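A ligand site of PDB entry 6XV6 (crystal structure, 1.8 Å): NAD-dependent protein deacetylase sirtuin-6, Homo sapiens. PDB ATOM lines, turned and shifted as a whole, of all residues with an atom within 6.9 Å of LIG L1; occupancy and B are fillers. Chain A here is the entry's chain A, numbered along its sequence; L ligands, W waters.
O10 of LG2 L2 is in hydrogen-bond range of O of Gln 111, 2.9 Å away. The side-chain carboxylate (OD2) of Asp 114 is in hydrogen-bond range of a nitrogen (N2) of LIG L1. O5 of LG2 L2 sits at hydrogen-bond distance from N of Phe 62 (2.9 Å). An oxygen (O1) of LIG L1 sits at hydrogen-bond distance from the backbone NH of Asp 114, at 3.1 Å. The side-chain hydroxyl of Thr 55 lies within hydrogen-bond range of a nitrogen (N4) of LG2 L2 (2.9 Å). N of Ala 51 sits at hydrogen-bond distance from O2 of LG2 L2 (2.8 Å). OH of Tyr 3 sits at hydrogen-bond distance from O7 of LG2 L2 (2.7 Å). N of Val 113 sits at hydrogen-bond distance from O1 of LIG L1, 3.0 Å away.
The side-chain carboxylate of Asp 114 sits at hydrogen-bond distance from the side-chain hydroxyl of Ser 54 (2.7 Å). N of Ala 51 is in hydrogen-bond range of OD1 of Asn 112 (3.0 Å). The backbone carbonyl oxygen of Phe 62 is in hydrogen-bond range of the backbone NH of Val 68 (3.3 Å). The backbone NH of Ile 59 lies within hydrogen-bond range of the backbone carbonyl oxygen of Ser 54 (3.3 Å). N of Leu 116 sits at hydrogen-bond distance from OD1 of Asp 114, at 3.0 Å. The backbone carbonyl oxygen (O) of Gly 50 sits at hydrogen-bond distance from the side-chain amide nitrogen (ND2) of Asn 112 (3.0 Å). The backbone carbonyl oxygen (O) of Val 113 sits at hydrogen-bond distance from the backbone NH (N) of Met 134, 2.9 Å away.
The backbone carbonyl oxygen (O) of Pro 60 lies close to a nitrogen (N1) of LIG L1, at 2.9 Å. Merely in contact with LIG L1: Tyr 3 (3.7 Å), Ala 51 (3.9 Å), Ile 59 (3.6 Å), Phe 62 (3.6 Å), Phe 84 (3.98 Å) and Asn 112 (3.6 Å). Hydrophobic or aromatic side chains that line LIG L1: Tyr 3, Ala 51, Ile 59, Phe 62, Phe 84 and Val 113. Nine residues have an atom within 4 Å of LIG L1: Tyr 3, Ala 51, Ile 59, Pro 60, Phe 62, Phe 84, Asn 112, Val 113 and Asp 114.
Water W2 lies within hydrogen-bond range of the backbone carbonyl oxygen (O) of Gln 111 (3.1 Å), the backbone NH (N) of Val 113 (3.1 Å), an oxygen (O1) of LIG L1 (3.2 Å) and an oxygen (O10) of LG2 L2 (3.4 Å).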
ATOM      1  N   TYR A   3      -3.877   8.394 -26.722  1.00  0.00           N
ATOM      2  CA  TYR A   3      -3.925   9.875 -26.795  1.00  0.00           C
ATOM      3  C   TYR A   3      -4.015  10.456 -25.382  1.00  0.00           C
ATOM      4  O   TYR A   3      -3.247  11.368 -25.028  1.00  0.00           O
ATOM      5  CB  TYR A   3      -5.124  10.366 -27.615  1.00  0.00           C
ATOM      6  CG  TYR A   3      -5.182  11.849 -27.895  1.00  0.00           C
ATOM      7  CD1 TYR A   3      -4.056  12.613 -28.182  1.00  0.00           C
ATOM      8  CD2 TYR A   3      -6.411  12.470 -27.976  1.00  0.00           C
ATOM      9  CE1 TYR A   3      -4.166  13.952 -28.513  1.00  0.00           C
ATOM     10  CE2 TYR A   3      -6.538  13.820 -28.297  1.00  0.00           C
ATOM     11  CZ  TYR A   3      -5.415  14.571 -28.586  1.00  0.00           C
ATOM     12  OH  TYR A   3      -5.598  15.891 -28.911  1.00  0.00           O
ATOM     13  N   ALA A   4      -4.932   9.878 -24.615  1.00  0.00           N
ATOM     14  CA  ALA A   4      -5.138  10.263 -23.215  1.00  0.00           C
ATOM     15  C   ALA A   4      -3.822  10.079 -22.459  1.00  0.00           C
ATOM     16  O   ALA A   4      -3.342  11.029 -21.873  1.00  0.00           O
ATOM     17  CB  ALA A   4      -6.239   9.420 -22.644  1.00  0.00           C
ATOM     18  N   GLY A  50     -15.954  19.501 -31.702  1.00  0.00           N
ATOM     19  CA  GLY A  50     -15.126  18.826 -30.702  1.00  0.00           C
ATOM     20  C   GLY A  50     -15.699  17.477 -30.366  1.00  0.00           C
ATOM     21  O   GLY A  50     -16.598  16.960 -31.125  1.00  0.00           O
ATOM     22  N   ALA A  51     -15.235  16.895 -29.267  1.00  0.00           N
ATOM     23  CA  ALA A  51     -15.396  15.452 -28.995  1.00  0.00           C
ATOM     24  C   ALA A  51     -16.861  15.106 -28.774  1.00  0.00           C
ATOM     25  O   ALA A  51     -17.232  13.916 -28.914  1.00  0.00           O
ATOM     26  CB  ALA A  51     -14.524  15.070 -27.821  1.00  0.00           C
ATOM     27  N   GLY A  52     -17.696  16.071 -28.434  1.00  0.00           N
ATOM     28  CA  GLY A  52     -19.105  15.794 -28.157  1.00  0.00           C
ATOM     29  C   GLY A  52     -19.863  15.307 -29.404  1.00  0.00           C
ATOM     30  O   GLY A  52     -20.950  14.721 -29.241  1.00  0.00           O
ATOM     31  N   ILE A  53     -19.361  15.556 -30.625  1.00  0.00           N
ATOM     32  CA  ILE A  53     -20.054  15.058 -31.847  1.00  0.00           C
ATOM     33  C   ILE A  53     -19.735  13.588 -32.111  1.00  0.00           C
ATOM     34  O   ILE A  53     -20.360  13.023 -33.043  1.00  0.00           O
ATOM     35  CB  ILE A  53     -19.808  15.928 -33.094  1.00  0.00           C
ATOM     36  CG1 ILE A  53     -18.394  15.801 -33.646  1.00  0.00           C
ATOM     37  CG2 ILE A  53     -20.180  17.397 -32.841  1.00  0.00           C
ATOM     38  CD1 ILE A  53     -18.298  16.073 -35.130  1.00  0.00           C
ATOM     39  N   SER A  54     -18.841  12.951 -31.354  1.00  0.00           N
ATOM     40  CA  SER A  54     -18.493  11.520 -31.557  1.00  0.00           C
ATOM     41  C   SER A  54     -18.925  10.657 -30.371  1.00  0.00           C
ATOM     42  O   SER A  54     -18.744   9.428 -30.437  1.00  0.00           O
ATOM     43  CB  SER A  54     -17.048  11.369 -31.883  1.00  0.00           C
ATOM     44  OG  SER A  54     -16.731  12.146 -33.025  1.00  0.00           O
ATOM     45  N   THR A  55     -19.499  11.240 -29.324  1.00  0.00           N
ATOM     46  CA  THR A  55     -19.923  10.450 -28.149  1.00  0.00           C
ATOM     47  C   THR A  55     -21.050   9.492 -28.556  1.00  0.00           C
ATOM     48  O   THR A  55     -21.038   8.364 -28.051  1.00  0.00           O
ATOM     49  CB  THR A  55     -20.313  11.346 -26.963  1.00  0.00           C
ATOM     50  OG1 THR A  55     -21.356  12.259 -27.342  1.00  0.00           O
ATOM     51  CG2 THR A  55     -19.108  12.082 -26.436  1.00  0.00           C
ATOM     52  N   ILE A  59     -17.354   6.986 -28.714  1.00  0.00           N
ATOM     53  CA  ILE A  59     -16.025   7.548 -28.355  1.00  0.00           C
ATOM     54  C   ILE A  59     -16.240   8.587 -27.260  1.00  0.00           C
ATOM     55  O   ILE A  59     -16.947   9.571 -27.481  1.00  0.00           O
ATOM     56  CB  ILE A  59     -15.357   8.168 -29.582  1.00  0.00           C
ATOM     57  CG1 ILE A  59     -15.237   7.156 -30.720  1.00  0.00           C
ATOM     58  CG2 ILE A  59     -14.021   8.814 -29.209  1.00  0.00           C
ATOM     59  CD1 ILE A  59     -14.669   7.729 -31.969  1.00  0.00           C
ATOM     60  N   PRO A  60     -15.613   8.433 -26.077  1.00  0.00           N
ATOM     61  CA  PRO A  60     -15.851   9.351 -24.963  1.00  0.00           C
ATOM     62  C   PRO A  60     -15.232  10.734 -25.235  1.00  0.00           C
ATOM     63  O   PRO A  60     -14.306  10.844 -26.025  1.00  0.00           O
ATOM     64  CB  PRO A  60     -15.156   8.627 -23.805  1.00  0.00           C
ATOM     65  CG  PRO A  60     -13.986   7.936 -24.489  1.00  0.00           C
ATOM     66  CD  PRO A  60     -14.590   7.408 -25.778  1.00  0.00           C
ATOM     67  N   ASP A  61     -15.776  11.771 -24.629  1.00  0.00           N
ATOM     68  CA  ASP A  61     -15.209  13.137 -24.683  1.00  0.00           C
ATOM     69  C   ASP A  61     -14.162  13.283 -23.576  1.00  0.00           C
ATOM     70  O   ASP A  61     -13.765  12.249 -22.985  1.00  0.00           O
ATOM     71  CB  ASP A  61     -16.323  14.173 -24.662  1.00  0.00           C
ATOM     72  CG  ASP A  61     -17.186  14.229 -23.421  1.00  0.00           C
ATOM     73  OD1 ASP A  61     -16.707  13.772 -22.358  1.00  0.00           O
ATOM     74  OD2 ASP A  61     -18.302  14.737 -23.520  1.00  0.00           O
ATOM     75  N   PHE A  62     -13.669  14.499 -23.340  1.00  0.00           N
ATOM     76  CA  PHE A  62     -12.588  14.759 -22.358  1.00  0.00           C
ATOM     77  C   PHE A  62     -13.165  15.248 -21.029  1.00  0.00           C
ATOM     78  O   PHE A  62     -12.667  14.810 -19.983  1.00  0.00           O
ATOM     79  CB  PHE A  62     -11.561  15.717 -22.950  1.00  0.00           C
ATOM     80  CG  PHE A  62     -10.795  15.120 -24.105  1.00  0.00           C
ATOM     81  CD1 PHE A  62      -9.673  14.350 -23.886  1.00  0.00           C
ATOM     82  CD2 PHE A  62     -11.267  15.278 -25.399  1.00  0.00           C
ATOM     83  CE1 PHE A  62      -8.997  13.774 -24.953  1.00  0.00           C
ATOM     84  CE2 PHE A  62     -10.598  14.680 -26.456  1.00  0.00           C
ATOM     85  CZ  PHE A  62      -9.481  13.918 -26.233  1.00  0.00           C
ATOM     86  N   VAL A  68     -12.729  11.556 -20.483  1.00  0.00           N
ATOM     87  CA  VAL A  68     -11.374  11.029 -20.125  1.00  0.00           C
ATOM     88  C   VAL A  68     -10.905  11.683 -18.819  1.00  0.00           C
ATOM     89  O   VAL A  68     -10.504  10.947 -17.924  1.00  0.00           O
ATOM     90  CB  VAL A  68     -10.364  11.286 -21.266  1.00  0.00           C
ATOM     91  CG1 VAL A  68      -9.004  10.727 -20.885  1.00  0.00           C
ATOM     92  CG2 VAL A  68     -10.818  10.659 -22.585  1.00  0.00           C
ATOM     93  N   PRO A  78     -11.475   5.890 -19.311  1.00  0.00           N
ATOM     94  CA  PRO A  78     -12.634   6.233 -20.135  1.00  0.00           C
ATOM     95  C   PRO A  78     -13.126   4.909 -20.760  1.00  0.00           C
ATOM     96  O   PRO A  78     -12.366   3.998 -20.878  1.00  0.00           O
ATOM     97  CB  PRO A  78     -12.067   7.227 -21.141  1.00  0.00           C
ATOM     98  CG  PRO A  78     -10.619   6.830 -21.275  1.00  0.00           C
ATOM     99  CD  PRO A  78     -10.214   6.359 -19.895  1.00  0.00           C
ATOM    100  N   PHE A  80     -14.723   3.182 -24.151  1.00  0.00           N
ATOM    101  CA  PHE A  80     -15.020   3.137 -25.596  1.00  0.00           C
ATOM    102  C   PHE A  80     -16.069   2.054 -25.818  1.00  0.00           C
ATOM    103  O   PHE A  80     -15.912   0.946 -25.283  1.00  0.00           O
ATOM    104  CB  PHE A  80     -13.743   2.860 -26.374  1.00  0.00           C
ATOM    105  CG  PHE A  80     -12.836   4.044 -26.524  1.00  0.00           C
ATOM    106  CD1 PHE A  80     -12.066   4.495 -25.456  1.00  0.00           C
ATOM    107  CD2 PHE A  80     -12.702   4.690 -27.747  1.00  0.00           C
ATOM    108  CE1 PHE A  80     -11.205   5.566 -25.609  1.00  0.00           C
ATOM    109  CE2 PHE A  80     -11.830   5.765 -27.893  1.00  0.00           C
ATOM    110  CZ  PHE A  80     -11.079   6.192 -26.822  1.00  0.00           C
ATOM    111  N   PHE A  84     -11.452   3.040 -32.891  1.00  0.00           N
ATOM    112  CA  PHE A  84     -11.419   4.140 -33.877  1.00  0.00           C
ATOM    113  C   PHE A  84     -11.732   3.588 -35.264  1.00  0.00           C
ATOM    114  O   PHE A  84     -12.468   4.252 -36.017  1.00  0.00           O
ATOM    115  CB  PHE A  84     -10.072   4.853 -33.827  1.00  0.00           C
ATOM    116  CG  PHE A  84      -9.901   5.719 -32.602  1.00  0.00           C
ATOM    117  CD1 PHE A  84     -10.645   6.866 -32.464  1.00  0.00           C
ATOM    118  CD2 PHE A  84      -8.929   5.439 -31.661  1.00  0.00           C
ATOM    119  CE1 PHE A  84     -10.493   7.690 -31.361  1.00  0.00           C
ATOM    120  CE2 PHE A  84      -8.756   6.252 -30.559  1.00  0.00           C
ATOM    121  CZ  PHE A  84      -9.524   7.397 -30.422  1.00  0.00           C
ATOM    122  N   GLN A 111     -11.330  19.942 -33.597  1.00  0.00           N
ATOM    123  CA  GLN A 111     -10.307  19.578 -32.596  1.00  0.00           C
ATOM    124  C   GLN A 111     -10.189  18.062 -32.494  1.00  0.00           C
ATOM    125  O   GLN A 111      -9.295  17.611 -31.766  1.00  0.00           O
ATOM    126  CB  GLN A 111     -10.729  20.220 -31.271  1.00  0.00           C
ATOM    127  CG  GLN A 111     -10.700  21.725 -31.328  1.00  0.00           C
ATOM    128  CD  GLN A 111     -11.312  22.313 -30.097  1.00  0.00           C
ATOM    129  OE1 GLN A 111     -10.708  22.255 -29.018  1.00  0.00           O
ATOM    130  NE2 GLN A 111     -12.529  22.821 -30.241  1.00  0.00           N
ATOM    131  N   ASN A 112     -11.035  17.300 -33.193  1.00  0.00           N
ATOM    132  CA  ASN A 112     -11.114  15.834 -33.040  1.00  0.00           C
ATOM    133  C   ASN A 112      -9.971  15.141 -33.779  1.00  0.00           C
ATOM    134  O   ASN A 112      -9.736  15.471 -34.945  1.00  0.00           O
ATOM    135  CB  ASN A 112     -12.461  15.288 -33.511  1.00  0.00           C
ATOM    136  CG  ASN A 112     -13.601  15.762 -32.640  1.00  0.00           C
ATOM    137  OD1 ASN A 112     -13.367  16.274 -31.538  1.00  0.00           O
ATOM    138  ND2 ASN A 112     -14.822  15.618 -33.127  1.00  0.00           N
ATOM    139  N   VAL A 113      -9.334  14.167 -33.125  1.00  0.00           N
ATOM    140  CA  VAL A 113      -8.296  13.312 -33.752  1.00  0.00           C
ATOM    141  C   VAL A 113      -8.924  11.983 -34.209  1.00  0.00           C
ATOM    142  O   VAL A 113      -8.165  11.162 -34.719  1.00  0.00           O
ATOM    143  CB  VAL A 113      -7.091  13.099 -32.800  1.00  0.00           C
ATOM    144  CG1 VAL A 113      -6.449  14.407 -32.387  1.00  0.00           C
ATOM    145  CG2 VAL A 113      -7.491  12.307 -31.591  1.00  0.00           C
ATOM    146  N   ASP A 114     -10.210  11.764 -34.017  1.00  0.00           N
ATOM    147  CA  ASP A 114     -10.891  10.452 -34.225  1.00  0.00           C
ATOM    148  C   ASP A 114     -10.977  10.068 -35.720  1.00  0.00           C
ATOM    149  O   ASP A 114     -11.350   8.929 -36.004  1.00  0.00           O
ATOM    150  CB  ASP A 114     -12.284  10.441 -33.588  1.00  0.00           C
ATOM    151  CG  ASP A 114     -13.231  11.526 -34.086  1.00  0.00           C
ATOM    152  OD1 ASP A 114     -13.161  11.909 -35.302  1.00  0.00           O
ATOM    153  OD2 ASP A 114     -14.029  11.995 -33.265  1.00  0.00           O
ATOM    154  N   GLY A 115     -10.631  10.956 -36.664  1.00  0.00           N
ATOM    155  CA  GLY A 115     -10.584  10.651 -38.112  1.00  0.00           C
ATOM    156  C   GLY A 115     -11.960  10.524 -38.750  1.00  0.00           C
ATOM    157  O   GLY A 115     -12.014  10.146 -39.947  1.00  0.00           O
ATOM    158  N   LEU A 116     -13.048  10.820 -38.050  1.00  0.00           N
ATOM    159  CA  LEU A 116     -14.409  10.544 -38.559  1.00  0.00           C
ATOM    160  C   LEU A 116     -14.844  11.568 -39.612  1.00  0.00           C
ATOM    161  O   LEU A 116     -15.582  11.197 -40.544  1.00  0.00           O
ATOM    162  CB  LEU A 116     -15.382  10.480 -37.384  1.00  0.00           C
ATOM    163  CG  LEU A 116     -15.317   9.184 -36.580  1.00  0.00           C
ATOM    164  CD1 LEU A 116     -16.235   9.285 -35.373  1.00  0.00           C
ATOM    165  CD2 LEU A 116     -15.748   7.994 -37.449  1.00  0.00           C
ATOM    166  N   MET A 134      -5.729  10.603 -36.136  1.00  0.00           N
ATOM    167  CA  MET A 134      -5.111   9.325 -35.681  1.00  0.00           C
ATOM    168  C   MET A 134      -4.754   8.477 -36.909  1.00  0.00           C
ATOM    169  O   MET A 134      -3.858   7.607 -36.757  1.00  0.00           O
ATOM    170  CB  MET A 134      -6.069   8.533 -34.796  1.00  0.00           C
ATOM    171  CG  MET A 134      -6.298   9.156 -33.458  1.00  0.00           C
ATOM    172  SD  MET A 134      -6.386   8.048 -32.117  1.00  0.00           S
ATOM    173  CE  MET A 134      -4.626   7.754 -31.921  1.00  0.00           C
HETATM  174  N1  LIG L   1     -11.537  11.011 -26.739  1.00  0.00           N
HETATM  175  C1  LIG L   1     -12.077  11.593 -27.882  1.00  0.00           C
HETATM  176  C2  LIG L   1     -11.350  11.676 -29.079  1.00  0.00           C
HETATM  177  C3  LIG L   1     -10.065  11.131 -29.095  1.00  0.00           C
HETATM  178  C4  LIG L   1      -9.515  10.517 -27.952  1.00  0.00           C
HETATM  179  C5  LIG L   1     -10.279  10.460 -26.777  1.00  0.00           C
HETATM  180  C6  LIG L   1     -11.959  12.334 -30.366  1.00  0.00           C
HETATM  181  O1  LIG L   1     -11.176  12.736 -31.244  1.00  0.00           O
HETATM  182  N2  LIG L   1     -13.327  12.481 -30.562  1.00  0.00           N
HETATM  183  N1  LG2 L   2     -24.430  16.574 -27.625  1.00  0.00           N
HETATM  184  C1  LG2 L   2     -24.015  17.777 -27.213  1.00  0.00           C
HETATM  185  N2  LG2 L   2     -22.981  18.097 -26.420  1.00  0.00           N
HETATM  186  C2  LG2 L   2     -22.290  16.988 -26.083  1.00  0.00           C
HETATM  187  C3  LG2 L   2     -22.586  15.687 -26.456  1.00  0.00           C
HETATM  188  C4  LG2 L   2     -23.724  15.474 -27.259  1.00  0.00           C
HETATM  189  N3  LG2 L   2     -24.101  14.267 -27.722  1.00  0.00           N
HETATM  190  N4  LG2 L   2     -21.648  14.812 -25.912  1.00  0.00           N
HETATM  191  C5  LG2 L   2     -20.818  15.591 -25.269  1.00  0.00           C
HETATM  192  N5  LG2 L   2     -21.165  16.922 -25.309  1.00  0.00           N
HETATM  193  P1  LG2 L   2     -14.499  18.445 -24.285  1.00  0.00           P
HETATM  194  P2  LG2 L   2     -13.202  19.217 -26.742  1.00  0.00           P
HETATM  195  C6  LG2 L   2     -20.397  18.043 -24.790  1.00  0.00           C
HETATM  196  O1  LG2 L   2     -13.735  19.553 -23.633  1.00  0.00           O
HETATM  197  O2  LG2 L   2     -13.257  18.588 -28.123  1.00  0.00           O
HETATM  198  C7  LG2 L   2      -8.136  17.811 -25.437  1.00  0.00           C
HETATM  199  O3  LG2 L   2      -6.880  18.147 -24.838  1.00  0.00           O
HETATM  200  C8  LG2 L   2     -19.868  17.895 -23.364  1.00  0.00           C
HETATM  201  O4  LG2 L   2     -20.827  18.420 -22.484  1.00  0.00           O
HETATM  202  O5  LG2 L   2     -14.723  17.134 -23.648  1.00  0.00           O
HETATM  203  O6  LG2 L   2     -13.818  20.562 -26.552  1.00  0.00           O
HETATM  204  C9  LG2 L   2      -8.012  17.403 -26.918  1.00  0.00           C
HETATM  205  O7  LG2 L   2      -6.867  17.930 -27.584  1.00  0.00           O
HETATM  206  C10 LG2 L   2     -18.561  18.706 -23.387  1.00  0.00           C
HETATM  207  O8  LG2 L   2     -18.683  19.993 -22.802  1.00  0.00           O
HETATM  208  O9  LG2 L   2     -13.853  18.184 -25.729  1.00  0.00           O
HETATM  209  C11 LG2 L   2      -9.291  17.966 -27.533  1.00  0.00           C
HETATM  210  O10 LG2 L   2      -9.259  18.159 -28.950  1.00  0.00           O
HETATM  211  C12 LG2 L   2     -18.248  18.888 -24.862  1.00  0.00           C
HETATM  212  O11 LG2 L   2     -19.241  18.133 -25.573  1.00  0.00           O
HETATM  213  C13 LG2 L   2      -9.344  19.308 -26.790  1.00  0.00           C
HETATM  214  O12 LG2 L   2      -8.962  18.968 -25.428  1.00  0.00           O
HETATM  215  C14 LG2 L   2     -16.911  18.380 -25.303  1.00  0.00           C
HETATM  216  O13 LG2 L   2     -15.891  19.133 -24.637  1.00  0.00           O
HETATM  217  C15 LG2 L   2     -10.670  20.026 -26.798  1.00  0.00           C
HETATM  218  O14 LG2 L   2     -11.683  19.195 -26.196  1.00  0.00           O
HETATM  219  O   HOH W   1     -15.580  11.841 -28.783  1.00  0.00           O
HETATM  220  O   HOH W   2      -9.149  14.990 -30.128  1.00  0.00           O
